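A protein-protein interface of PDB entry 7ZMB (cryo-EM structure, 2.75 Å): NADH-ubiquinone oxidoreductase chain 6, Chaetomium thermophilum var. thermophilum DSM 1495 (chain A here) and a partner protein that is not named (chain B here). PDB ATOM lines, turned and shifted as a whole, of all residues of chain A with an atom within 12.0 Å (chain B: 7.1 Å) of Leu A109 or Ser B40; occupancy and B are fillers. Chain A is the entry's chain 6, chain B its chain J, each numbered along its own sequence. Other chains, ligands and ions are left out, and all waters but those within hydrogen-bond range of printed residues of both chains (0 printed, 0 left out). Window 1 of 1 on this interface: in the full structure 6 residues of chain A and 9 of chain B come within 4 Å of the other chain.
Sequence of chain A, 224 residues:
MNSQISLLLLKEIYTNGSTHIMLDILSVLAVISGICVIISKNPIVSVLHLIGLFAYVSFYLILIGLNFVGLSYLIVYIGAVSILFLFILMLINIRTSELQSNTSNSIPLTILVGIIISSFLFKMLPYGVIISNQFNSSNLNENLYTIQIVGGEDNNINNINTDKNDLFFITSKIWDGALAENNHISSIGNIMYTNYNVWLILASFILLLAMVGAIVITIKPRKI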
ATOM      1  N   ILE A  38     -18.594 -16.080 -34.714  1.00  0.00           N
ATOM      2  CA  ILE A  38     -18.763 -15.083 -33.669  1.00  0.00           C
ATOM      3  C   ILE A  38     -17.452 -14.466 -33.204  1.00  0.00           C
ATOM      4  O   ILE A  38     -17.470 -13.327 -32.712  1.00  0.00           O
ATOM      5  CB  ILE A  38     -19.544 -15.658 -32.470  1.00  0.00           C
ATOM      6  CG1 ILE A  38     -18.891 -16.940 -31.966  1.00  0.00           C
ATOM      7  CG2 ILE A  38     -20.986 -15.936 -32.866  1.00  0.00           C
ATOM      8  CD1 ILE A  38     -19.663 -17.626 -30.889  1.00  0.00           C
ATOM      9  N   SER A 101     -12.720  -4.260 -31.603  1.00  0.00           N
ATOM     10  CA  SER A 101     -12.062  -5.312 -30.841  1.00  0.00           C
ATOM     11  C   SER A 101     -12.776  -5.555 -29.518  1.00  0.00           C
ATOM     12  O   SER A 101     -13.295  -4.628 -28.891  1.00  0.00           O
ATOM     13  CB  SER A 101     -10.597  -4.948 -30.591  1.00  0.00           C
ATOM     14  OG  SER A 101     -10.486  -3.763 -29.824  1.00  0.00           O
ATOM     15  N   ASN A 102     -12.795  -6.816 -29.095  1.00  0.00           N
ATOM     16  CA  ASN A 102     -13.453  -7.223 -27.865  1.00  0.00           C
ATOM     17  C   ASN A 102     -12.441  -7.891 -26.946  1.00  0.00           C
ATOM     18  O   ASN A 102     -11.458  -8.480 -27.401  1.00  0.00           O
ATOM     19  CB  ASN A 102     -14.621  -8.179 -28.138  1.00  0.00           C
ATOM     20  N   THR A 103     -12.693  -7.792 -25.644  1.00  0.00           N
ATOM     21  CA  THR A 103     -11.797  -8.330 -24.632  1.00  0.00           C
ATOM     22  C   THR A 103     -12.313  -9.680 -24.158  1.00  0.00           C
ATOM     23  O   THR A 103     -13.426 -10.099 -24.488  1.00  0.00           O
ATOM     24  CB  THR A 103     -11.654  -7.385 -23.434  1.00  0.00           C
ATOM     25  N   SER A 104     -11.481 -10.429 -23.442  1.00  0.00           N
ATOM     26  CA  SER A 104     -12.031 -11.705 -22.913  1.00  0.00           C
ATOM     27  C   SER A 104     -12.356 -11.567 -21.425  1.00  0.00           C
ATOM     28  O   SER A 104     -11.859 -12.389 -20.630  1.00  0.00           O
ATOM     29  CB  SER A 104     -11.105 -12.855 -23.157  1.00  0.00           C
ATOM     30  N   ASN A 105     -13.179 -10.575 -21.063  1.00  0.00           N
ATOM     31  CA  ASN A 105     -13.636 -10.468 -19.651  1.00  0.00           C
ATOM     32  C   ASN A 105     -14.784 -11.470 -19.512  1.00  0.00           C
ATOM     33  O   ASN A 105     -15.163 -11.785 -18.377  1.00  0.00           O
ATOM     34  CB  ASN A 105     -13.997  -9.028 -19.272  1.00  0.00           C
ATOM     35  CG  ASN A 105     -15.149  -8.462 -20.073  1.00  0.00           C
ATOM     36  OD1 ASN A 105     -15.544  -9.030 -21.089  1.00  0.00           O
ATOM     37  ND2 ASN A 105     -15.693  -7.341 -19.629  1.00  0.00           N
ATOM     38  N   SER A 106     -15.260 -11.992 -20.642  1.00  0.00           N
ATOM     39  CA  SER A 106     -16.428 -12.900 -20.625  1.00  0.00           C
ATOM     40  C   SER A 106     -16.000 -14.362 -20.718  1.00  0.00           C
ATOM     41  O   SER A 106     -16.908 -15.197 -20.741  1.00  0.00           O
ATOM     42  CB  SER A 106     -17.376 -12.543 -21.726  1.00  0.00           C
ATOM     43  OG  SER A 106     -16.704 -12.252 -22.930  1.00  0.00           O
ATOM     44  N   ILE A 107     -14.697 -14.656 -20.721  1.00  0.00           N
ATOM     45  CA  ILE A 107     -14.273 -16.052 -20.707  1.00  0.00           C
ATOM     46  C   ILE A 107     -14.739 -16.767 -19.442  1.00  0.00           C
ATOM     47  O   ILE A 107     -15.257 -17.887 -19.549  1.00  0.00           O
ATOM     48  CB  ILE A 107     -12.751 -16.173 -20.875  1.00  0.00           C
ATOM     49  CG1 ILE A 107     -12.320 -15.536 -22.192  1.00  0.00           C
ATOM     50  CG2 ILE A 107     -12.312 -17.629 -20.814  1.00  0.00           C
ATOM     51  CD1 ILE A 107     -12.934 -16.192 -23.404  1.00  0.00           C
ATOM     52  N   PRO A 108     -14.571 -16.208 -18.232  1.00  0.00           N
ATOM     53  CA  PRO A 108     -15.026 -16.960 -17.049  1.00  0.00           C
ATOM     54  C   PRO A 108     -16.516 -17.231 -17.047  1.00  0.00           C
ATOM     55  O   PRO A 108     -16.951 -18.280 -16.564  1.00  0.00           O
ATOM     56  CB  PRO A 108     -14.602 -16.076 -15.868  1.00  0.00           C
ATOM     57  CG  PRO A 108     -13.742 -15.022 -16.425  1.00  0.00           C
ATOM     58  CD  PRO A 108     -14.025 -14.891 -17.863  1.00  0.00           C
ATOM     59  N   LEU A 109     -17.317 -16.310 -17.575  1.00  0.00           N
ATOM     60  CA  LEU A 109     -18.739 -16.585 -17.719  1.00  0.00           C
ATOM     61  C   LEU A 109     -18.969 -17.698 -18.731  1.00  0.00           C
ATOM     62  O   LEU A 109     -19.830 -18.559 -18.530  1.00  0.00           O
ATOM     63  CB  LEU A 109     -19.477 -15.303 -18.111  1.00  0.00           C
ATOM     64  CG  LEU A 109     -21.004 -15.296 -18.153  1.00  0.00           C
ATOM     65  CD1 LEU A 109     -21.466 -13.895 -17.900  1.00  0.00           C
ATOM     66  CD2 LEU A 109     -21.537 -15.744 -19.492  1.00  0.00           C
ATOM     67  N   THR A 110     -18.191 -17.701 -19.818  1.00  0.00           N
ATOM     68  CA  THR A 110     -18.307 -18.735 -20.843  1.00  0.00           C
ATOM     69  C   THR A 110     -18.122 -20.128 -20.253  1.00  0.00           C
ATOM     70  O   THR A 110     -18.919 -21.037 -20.512  1.00  0.00           O
ATOM     71  CB  THR A 110     -17.271 -18.489 -21.943  1.00  0.00           C
ATOM     72  OG1 THR A 110     -17.321 -17.118 -22.361  1.00  0.00           O
ATOM     73  CG2 THR A 110     -17.517 -19.389 -23.125  1.00  0.00           C
ATOM     74  N   ILE A 111     -17.081 -20.304 -19.440  1.00  0.00           N
ATOM     75  CA  ILE A 111     -16.772 -21.621 -18.895  1.00  0.00           C
ATOM     76  C   ILE A 111     -17.904 -22.109 -18.002  1.00  0.00           C
ATOM     77  O   ILE A 111     -18.401 -23.230 -18.160  1.00  0.00           O
ATOM     78  CB  ILE A 111     -15.434 -21.584 -18.137  1.00  0.00           C
ATOM     79  CG1 ILE A 111     -14.350 -20.952 -19.008  1.00  0.00           C
ATOM     80  CG2 ILE A 111     -15.028 -22.985 -17.706  1.00  0.00           C
ATOM     81  CD1 ILE A 111     -14.076 -21.712 -20.284  1.00  0.00           C
ATOM     82  N   LEU A 112     -18.336 -21.271 -17.059  1.00  0.00           N
ATOM     83  CA  LEU A 112     -19.412 -21.654 -16.153  1.00  0.00           C
ATOM     84  C   LEU A 112     -20.714 -21.895 -16.908  1.00  0.00           C
ATOM     85  O   LEU A 112     -21.369 -22.927 -16.727  1.00  0.00           O
ATOM     86  CB  LEU A 112     -19.599 -20.571 -15.092  1.00  0.00           C
ATOM     87  CG  LEU A 112     -18.918 -20.763 -13.739  1.00  0.00           C
ATOM     88  CD1 LEU A 112     -19.124 -19.528 -12.884  1.00  0.00           C
ATOM     89  CD2 LEU A 112     -19.450 -21.999 -13.028  1.00  0.00           C
ATOM     90  N   VAL A 113     -21.104 -20.949 -17.764  1.00  0.00           N
ATOM     91  CA  VAL A 113     -22.334 -21.104 -18.535  1.00  0.00           C
ATOM     92  C   VAL A 113     -22.219 -22.269 -19.510  1.00  0.00           C
ATOM     93  O   VAL A 113     -23.198 -22.984 -19.752  1.00  0.00           O
ATOM     94  CB  VAL A 113     -22.675 -19.786 -19.257  1.00  0.00           C
ATOM     95  CG1 VAL A 113     -23.747 -20.002 -20.310  1.00  0.00           C
ATOM     96  CG2 VAL A 113     -23.124 -18.742 -18.253  1.00  0.00           C
ATOM     97  N   GLY A 114     -21.034 -22.487 -20.077  1.00  0.00           N
ATOM     98  CA  GLY A 114     -20.860 -23.613 -20.978  1.00  0.00           C
ATOM     99  C   GLY A 114     -21.052 -24.953 -20.292  1.00  0.00           C
ATOM    100  O   GLY A 114     -21.801 -25.805 -20.772  1.00  0.00           O
ATOM    101  N   ILE A 115     -20.384 -25.153 -19.155  1.00  0.00           N
ATOM    102  CA  ILE A 115     -20.411 -26.465 -18.515  1.00  0.00           C
ATOM    103  C   ILE A 115     -21.773 -26.739 -17.895  1.00  0.00           C
ATOM    104  O   ILE A 115     -22.278 -27.865 -17.950  1.00  0.00           O
ATOM    105  CB  ILE A 115     -19.274 -26.594 -17.482  1.00  0.00           C
ATOM    106  CG1 ILE A 115     -19.422 -25.572 -16.356  1.00  0.00           C
ATOM    107  CG2 ILE A 115     -17.919 -26.452 -18.158  1.00  0.00           C
ATOM    108  CD1 ILE A 115     -18.480 -25.800 -15.205  1.00  0.00           C
ATOM    109  N   ILE A 116     -22.390 -25.724 -17.296  1.00  0.00           N
ATOM    110  CA  ILE A 116     -23.615 -25.960 -16.544  1.00  0.00           C
ATOM    111  C   ILE A 116     -24.757 -26.343 -17.475  1.00  0.00           C
ATOM    112  O   ILE A 116     -25.512 -27.279 -17.190  1.00  0.00           O
ATOM    113  CB  ILE A 116     -23.949 -24.733 -15.677  1.00  0.00           C
ATOM    114  CG1 ILE A 116     -23.166 -24.810 -14.363  1.00  0.00           C
ATOM    115  CG2 ILE A 116     -25.439 -24.646 -15.417  1.00  0.00           C
ATOM    116  CD1 ILE A 116     -23.077 -23.510 -13.621  1.00  0.00           C
ATOM    117  N   ILE A 117     -24.897 -25.649 -18.606  1.00  0.00           N
ATOM    118  CA  ILE A 117     -25.938 -26.017 -19.563  1.00  0.00           C
ATOM    119  C   ILE A 117     -25.649 -27.393 -20.150  1.00  0.00           C
ATOM    120  O   ILE A 117     -26.526 -28.260 -20.208  1.00  0.00           O
ATOM    121  CB  ILE A 117     -26.072 -24.949 -20.662  1.00  0.00           C
ATOM    122  CG1 ILE A 117     -26.503 -23.616 -20.079  1.00  0.00           C
ATOM    123  CG2 ILE A 117     -27.150 -25.323 -21.621  1.00  0.00           C
ATOM    124  CD1 ILE A 117     -26.412 -22.474 -21.043  1.00  0.00           C
ATOM    125  N   SER A 118     -24.396 -27.626 -20.553  1.00  0.00           N
ATOM    126  CA  SER A 118     -24.037 -28.882 -21.202  1.00  0.00           C
ATOM    127  C   SER A 118     -24.245 -30.074 -20.279  1.00  0.00           C
ATOM    128  O   SER A 118     -24.711 -31.132 -20.714  1.00  0.00           O
ATOM    129  CB  SER A 118     -22.589 -28.826 -21.680  1.00  0.00           C
ATOM    130  OG  SER A 118     -21.751 -28.305 -20.672  1.00  0.00           O
ATOM    131  N   LEU B  33     -20.956 -17.292 -10.343  1.00  0.00           N
ATOM    132  CA  LEU B  33     -21.403 -16.862 -11.663  1.00  0.00           C
ATOM    133  C   LEU B  33     -21.887 -15.417 -11.654  1.00  0.00           C
ATOM    134  O   LEU B  33     -21.675 -14.688 -12.627  1.00  0.00           O
ATOM    135  CB  LEU B  33     -22.493 -17.794 -12.192  1.00  0.00           C
ATOM    136  CG  LEU B  33     -23.888 -17.849 -11.576  1.00  0.00           C
ATOM    137  CD1 LEU B  33     -24.812 -16.858 -12.267  1.00  0.00           C
ATOM    138  CD2 LEU B  33     -24.435 -19.248 -11.677  1.00  0.00           C
ATOM    139  N   ALA B  35     -20.509 -13.245  -9.896  1.00  0.00           N
ATOM    140  CA  ALA B  35     -19.214 -12.604 -10.090  1.00  0.00           C
ATOM    141  C   ALA B  35     -18.797 -12.632 -11.558  1.00  0.00           C
ATOM    142  O   ALA B  35     -18.293 -11.635 -12.084  1.00  0.00           O
ATOM    143  CB  ALA B  35     -18.164 -13.286  -9.219  1.00  0.00           C
ATOM    144  N   ALA B  36     -19.074 -13.735 -12.250  1.00  0.00           N
ATOM    145  CA  ALA B  36     -18.570 -13.846 -13.645  1.00  0.00           C
ATOM    146  C   ALA B  36     -19.370 -12.874 -14.495  1.00  0.00           C
ATOM    147  O   ALA B  36     -18.774 -12.275 -15.400  1.00  0.00           O
ATOM    148  CB  ALA B  36     -18.718 -15.251 -14.155  1.00  0.00           C
ATOM    149  N   VAL B  37     -20.670 -12.752 -14.210  1.00  0.00           N
ATOM    150  CA  VAL B  37     -21.557 -11.819 -14.937  1.00  0.00           C
ATOM    151  C   VAL B  37     -21.075 -10.390 -14.697  1.00  0.00           C
ATOM    152  O   VAL B  37     -21.091  -9.613 -15.648  1.00  0.00           O
ATOM    153  CB  VAL B  37     -23.000 -12.015 -14.465  1.00  0.00           C
ATOM    154  CG1 VAL B  37     -23.899 -10.904 -14.957  1.00  0.00           C
ATOM    155  CG2 VAL B  37     -23.528 -13.373 -14.889  1.00  0.00           C
ATOM    156  N   ARG B  38     -20.637 -10.073 -13.478  1.00  0.00           N
ATOM    157  CA  ARG B  38     -20.088  -8.718 -13.186  1.00  0.00           C
ATOM    158  C   ARG B  38     -18.842  -8.461 -14.060  1.00  0.00           C
ATOM    159  O   ARG B  38     -18.761  -7.351 -14.654  1.00  0.00           O
ATOM    160  CB  ARG B  38     -19.816  -8.604 -11.685  1.00  0.00           C
ATOM    161  CG  ARG B  38     -19.303  -7.251 -11.215  1.00  0.00           C
ATOM    162  CD  ARG B  38     -20.371  -6.177 -11.218  1.00  0.00           C
ATOM    163  NE  ARG B  38     -19.813  -4.894 -10.818  1.00  0.00           N
ATOM    164  CZ  ARG B  38     -19.789  -4.436  -9.573  1.00  0.00           C
ATOM    165  NH1 ARG B  38     -20.309  -5.150  -8.589  1.00  0.00           N
ATOM    166  NH2 ARG B  38     -19.248  -3.257  -9.319  1.00  0.00           N
ATOM    167  N   THR B  39     -17.952  -9.447 -14.185  1.00  0.00           N
ATOM    168  CA  THR B  39     -16.728  -9.273 -14.995  1.00  0.00           C
ATOM    169  C   THR B  39     -17.121  -9.022 -16.448  1.00  0.00           C
ATOM    170  O   THR B  39     -16.518  -8.144 -17.054  1.00  0.00           O
ATOM    171  CB  THR B  39     -15.853 -10.526 -14.989  1.00  0.00           C
ATOM    172  OG1 THR B  39     -15.974 -11.123 -13.705  1.00  0.00           O
ATOM    173  CG2 THR B  39     -14.406 -10.239 -15.317  1.00  0.00           C
ATOM    174  N   SER B  40     -18.098  -9.765 -16.962  1.00  0.00           N
ATOM    175  CA  SER B  40     -18.517  -9.622 -18.381  1.00  0.00           C
ATOM    176  C   SER B  40     -19.100  -8.230 -18.636  1.00  0.00           C
ATOM    177  O   SER B  40     -18.836  -7.673 -19.702  1.00  0.00           O
ATOM    178  CB  SER B  40     -19.485 -10.690 -18.767  1.00  0.00           C
ATOM    179  OG  SER B  40     -20.663 -10.597 -17.993  1.00  0.00           O
ATOM    180  N   LEU B  41     -19.865  -7.693 -17.690  1.00  0.00           N
ATOM    181  CA  LEU B  41     -20.547  -6.397 -17.940  1.00  0.00           C
ATOM    182  C   LEU B  41     -19.592  -5.233 -17.667  1.00  0.00           C
ATOM    183  O   LEU B  41     -20.013  -4.087 -17.875  1.00  0.00           O
ATOM    184  CB  LEU B  41     -21.816  -6.317 -17.091  1.00  0.00           C
ATOM    185  CG  LEU B  41     -22.880  -7.349 -17.444  1.00  0.00           C
ATOM    186  CD1 LEU B  41     -24.144  -7.142 -16.621  1.00  0.00           C
ATOM    187  CD2 LEU B  41     -23.193  -7.301 -18.930  1.00  0.00           C
ATOM    188  N   ALA B  42     -18.363  -5.516 -17.233  1.00  0.00           N
ATOM    189  CA  ALA B  42     -17.354  -4.458 -17.007  1.00  0.00           C
ATOM    190  C   ALA B  42     -17.044  -3.736 -18.319  1.00  0.00           C
ATOM    191  O   ALA B  42     -16.961  -4.415 -19.367  1.00  0.00           O
ATOM    192  CB  ALA B  42     -16.119  -5.054 -16.410  1.00  0.00           C
ATOM    193  N   ARG B  43     -16.880  -2.410 -18.263  1.00  0.00           N
ATOM    194  CA  ARG B  43     -16.621  -1.601 -19.488  1.00  0.00           C
ATOM    195  C   ARG B  43     -15.117  -1.481 -19.766  1.00  0.00           C
ATOM    196  O   ARG B  43     -14.761  -0.916 -20.814  1.00  0.00           O
ATOM    197  CB  ARG B  43     -17.243  -0.217 -19.309  1.00  0.00           C
ATOM    198  CG  ARG B  43     -18.763  -0.222 -19.316  1.00  0.00           C
ATOM    199  CD  ARG B  43     -19.351   1.157 -19.084  1.00  0.00           C
ATOM    200  NE  ARG B  43     -20.764   1.230 -19.430  1.00  0.00           N
ATOM    201  CZ  ARG B  43     -21.762   0.969 -18.591  1.00  0.00           C
ATOM    202  NH1 ARG B  43     -23.014   1.069 -19.002  1.00  0.00           N
ATOM    203  NH2 ARG B  43     -21.506   0.611 -17.345  1.00  0.00           N
ATOM    204  N   ILE B  51     -11.690 -12.459 -12.177  1.00  0.00           N
ATOM    205  CA  ILE B  51     -12.804 -13.068 -11.455  1.00  0.00           C
ATOM    206  C   ILE B  51     -12.506 -13.125  -9.961  1.00  0.00           C
ATOM    207  O   ILE B  51     -13.404 -12.951  -9.128  1.00  0.00           O
ATOM    208  CB  ILE B  51     -13.116 -14.462 -12.036  1.00  0.00           C
ATOM    209  CG1 ILE B  51     -14.303 -15.099 -11.310  1.00  0.00           C
ATOM    210  CG2 ILE B  51     -11.890 -15.364 -11.987  1.00  0.00           C
ATOM    211  CD1 ILE B  51     -15.622 -14.400 -11.574  1.00  0.00           C
ATOM    212  N   ASN B  55     -14.055  -9.437  -8.077  1.00  0.00           N
ATOM    213  CA  ASN B  55     -15.271 -10.216  -7.886  1.00  0.00           C
ATOM    214  C   ASN B  55     -15.131 -11.307  -6.838  1.00  0.00           C
ATOM    215  O   ASN B  55     -16.140 -11.927  -6.487  1.00  0.00           O
ATOM    216  CB  ASN B  55     -15.701 -10.839  -9.210  1.00  0.00           C
ATOM    217  CG  ASN B  55     -16.519  -9.906 -10.041  1.00  0.00           C
ATOM    218  OD1 ASN B  55     -17.296  -9.121  -9.513  1.00  0.00           O
ATOM    219  ND2 ASN B  55     -16.358  -9.980 -11.349  1.00  0.00           N
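The backbone carbonyl oxygen (O) of Thr B39 is in hydrogen-bond range of the side-chain amide nitrogen (ND2) of Asn A105 (2.8 Å). The side-chain amide nitrogen (ND2) of Asn A105 is in hydrogen-bond range of the backbone carbonyl oxygen (O) of Ala B42, 3.2 Å away. The backbone carbonyl oxygen (O) of Ser B40 lies within hydrogen-bond range of the side-chain amide nitrogen (ND2) of Asn A105, at 3.2 Å.
ND2 of Asn B55 sits at hydrogen-bond distance from OG1 of Thr B39, 2.6 Å away. OG1 of Thr B39 lies within hydrogen-bond range of O of Ala B35, 2.9 Å away. OG1 of Thr B39 lies close to O of Ala B36 (3.5 Å). The backbone carbonyl oxygen of Val B37 sits at hydrogen-bond distance from the side-chain hydroxyl of Ser B40, at 2.6 Å.
Leu A109 touches Ala B36. CD1 of Leu A109 touches CA of Val B37, at 3.6 Å. CD1 of Leu A109 touches OG of Ser B40, at 3.4 Å. CA of Leu B33 touches CD1 of Leu A112 (3.7 Å).
Printed residues of chain B within 4 Å of Leu A109: Ala B36 (3.8 Å), Val B37 (3.6 Å) and Ser B40 (3.4 Å). Thr A110 touches none of the printed residues of chain B. Of the printed residues of chain B, Leu A112 touches Leu B33. Printed residues of chain A within 4 Å of Leu B33: Leu A112. No residue of chain A comes within 4 Å of Leu B41. Ala B42 touches just one residue of chain A: Asn A105 (3.2 Å). The nearest residue of chain B that does not touch Leu A109 is Leu B33 (5.3 Å). The nearest residue of chain A that does not touch Ser B40 is Ser A106 (4.1 Å). The nearest printed residue of chain B that does not touch Leu A112 is Ala B36 (4.5 Å).
Printed residues of chain A that touch a printed residue of chain B: Asn A105, Leu A109 and Leu A112. Hydrophobic or aromatic side chains of chain B within 4 Å of the printed part of chain A: Leu B33, Ala B36, Val B37 and Ala B42. Among the printed residues, 7 pairs touch across the chains. Among the printed residues, no Asp or Glu carboxylate lies within 4 Å of a Lys or Arg side-chain nitrogen of the other chain.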
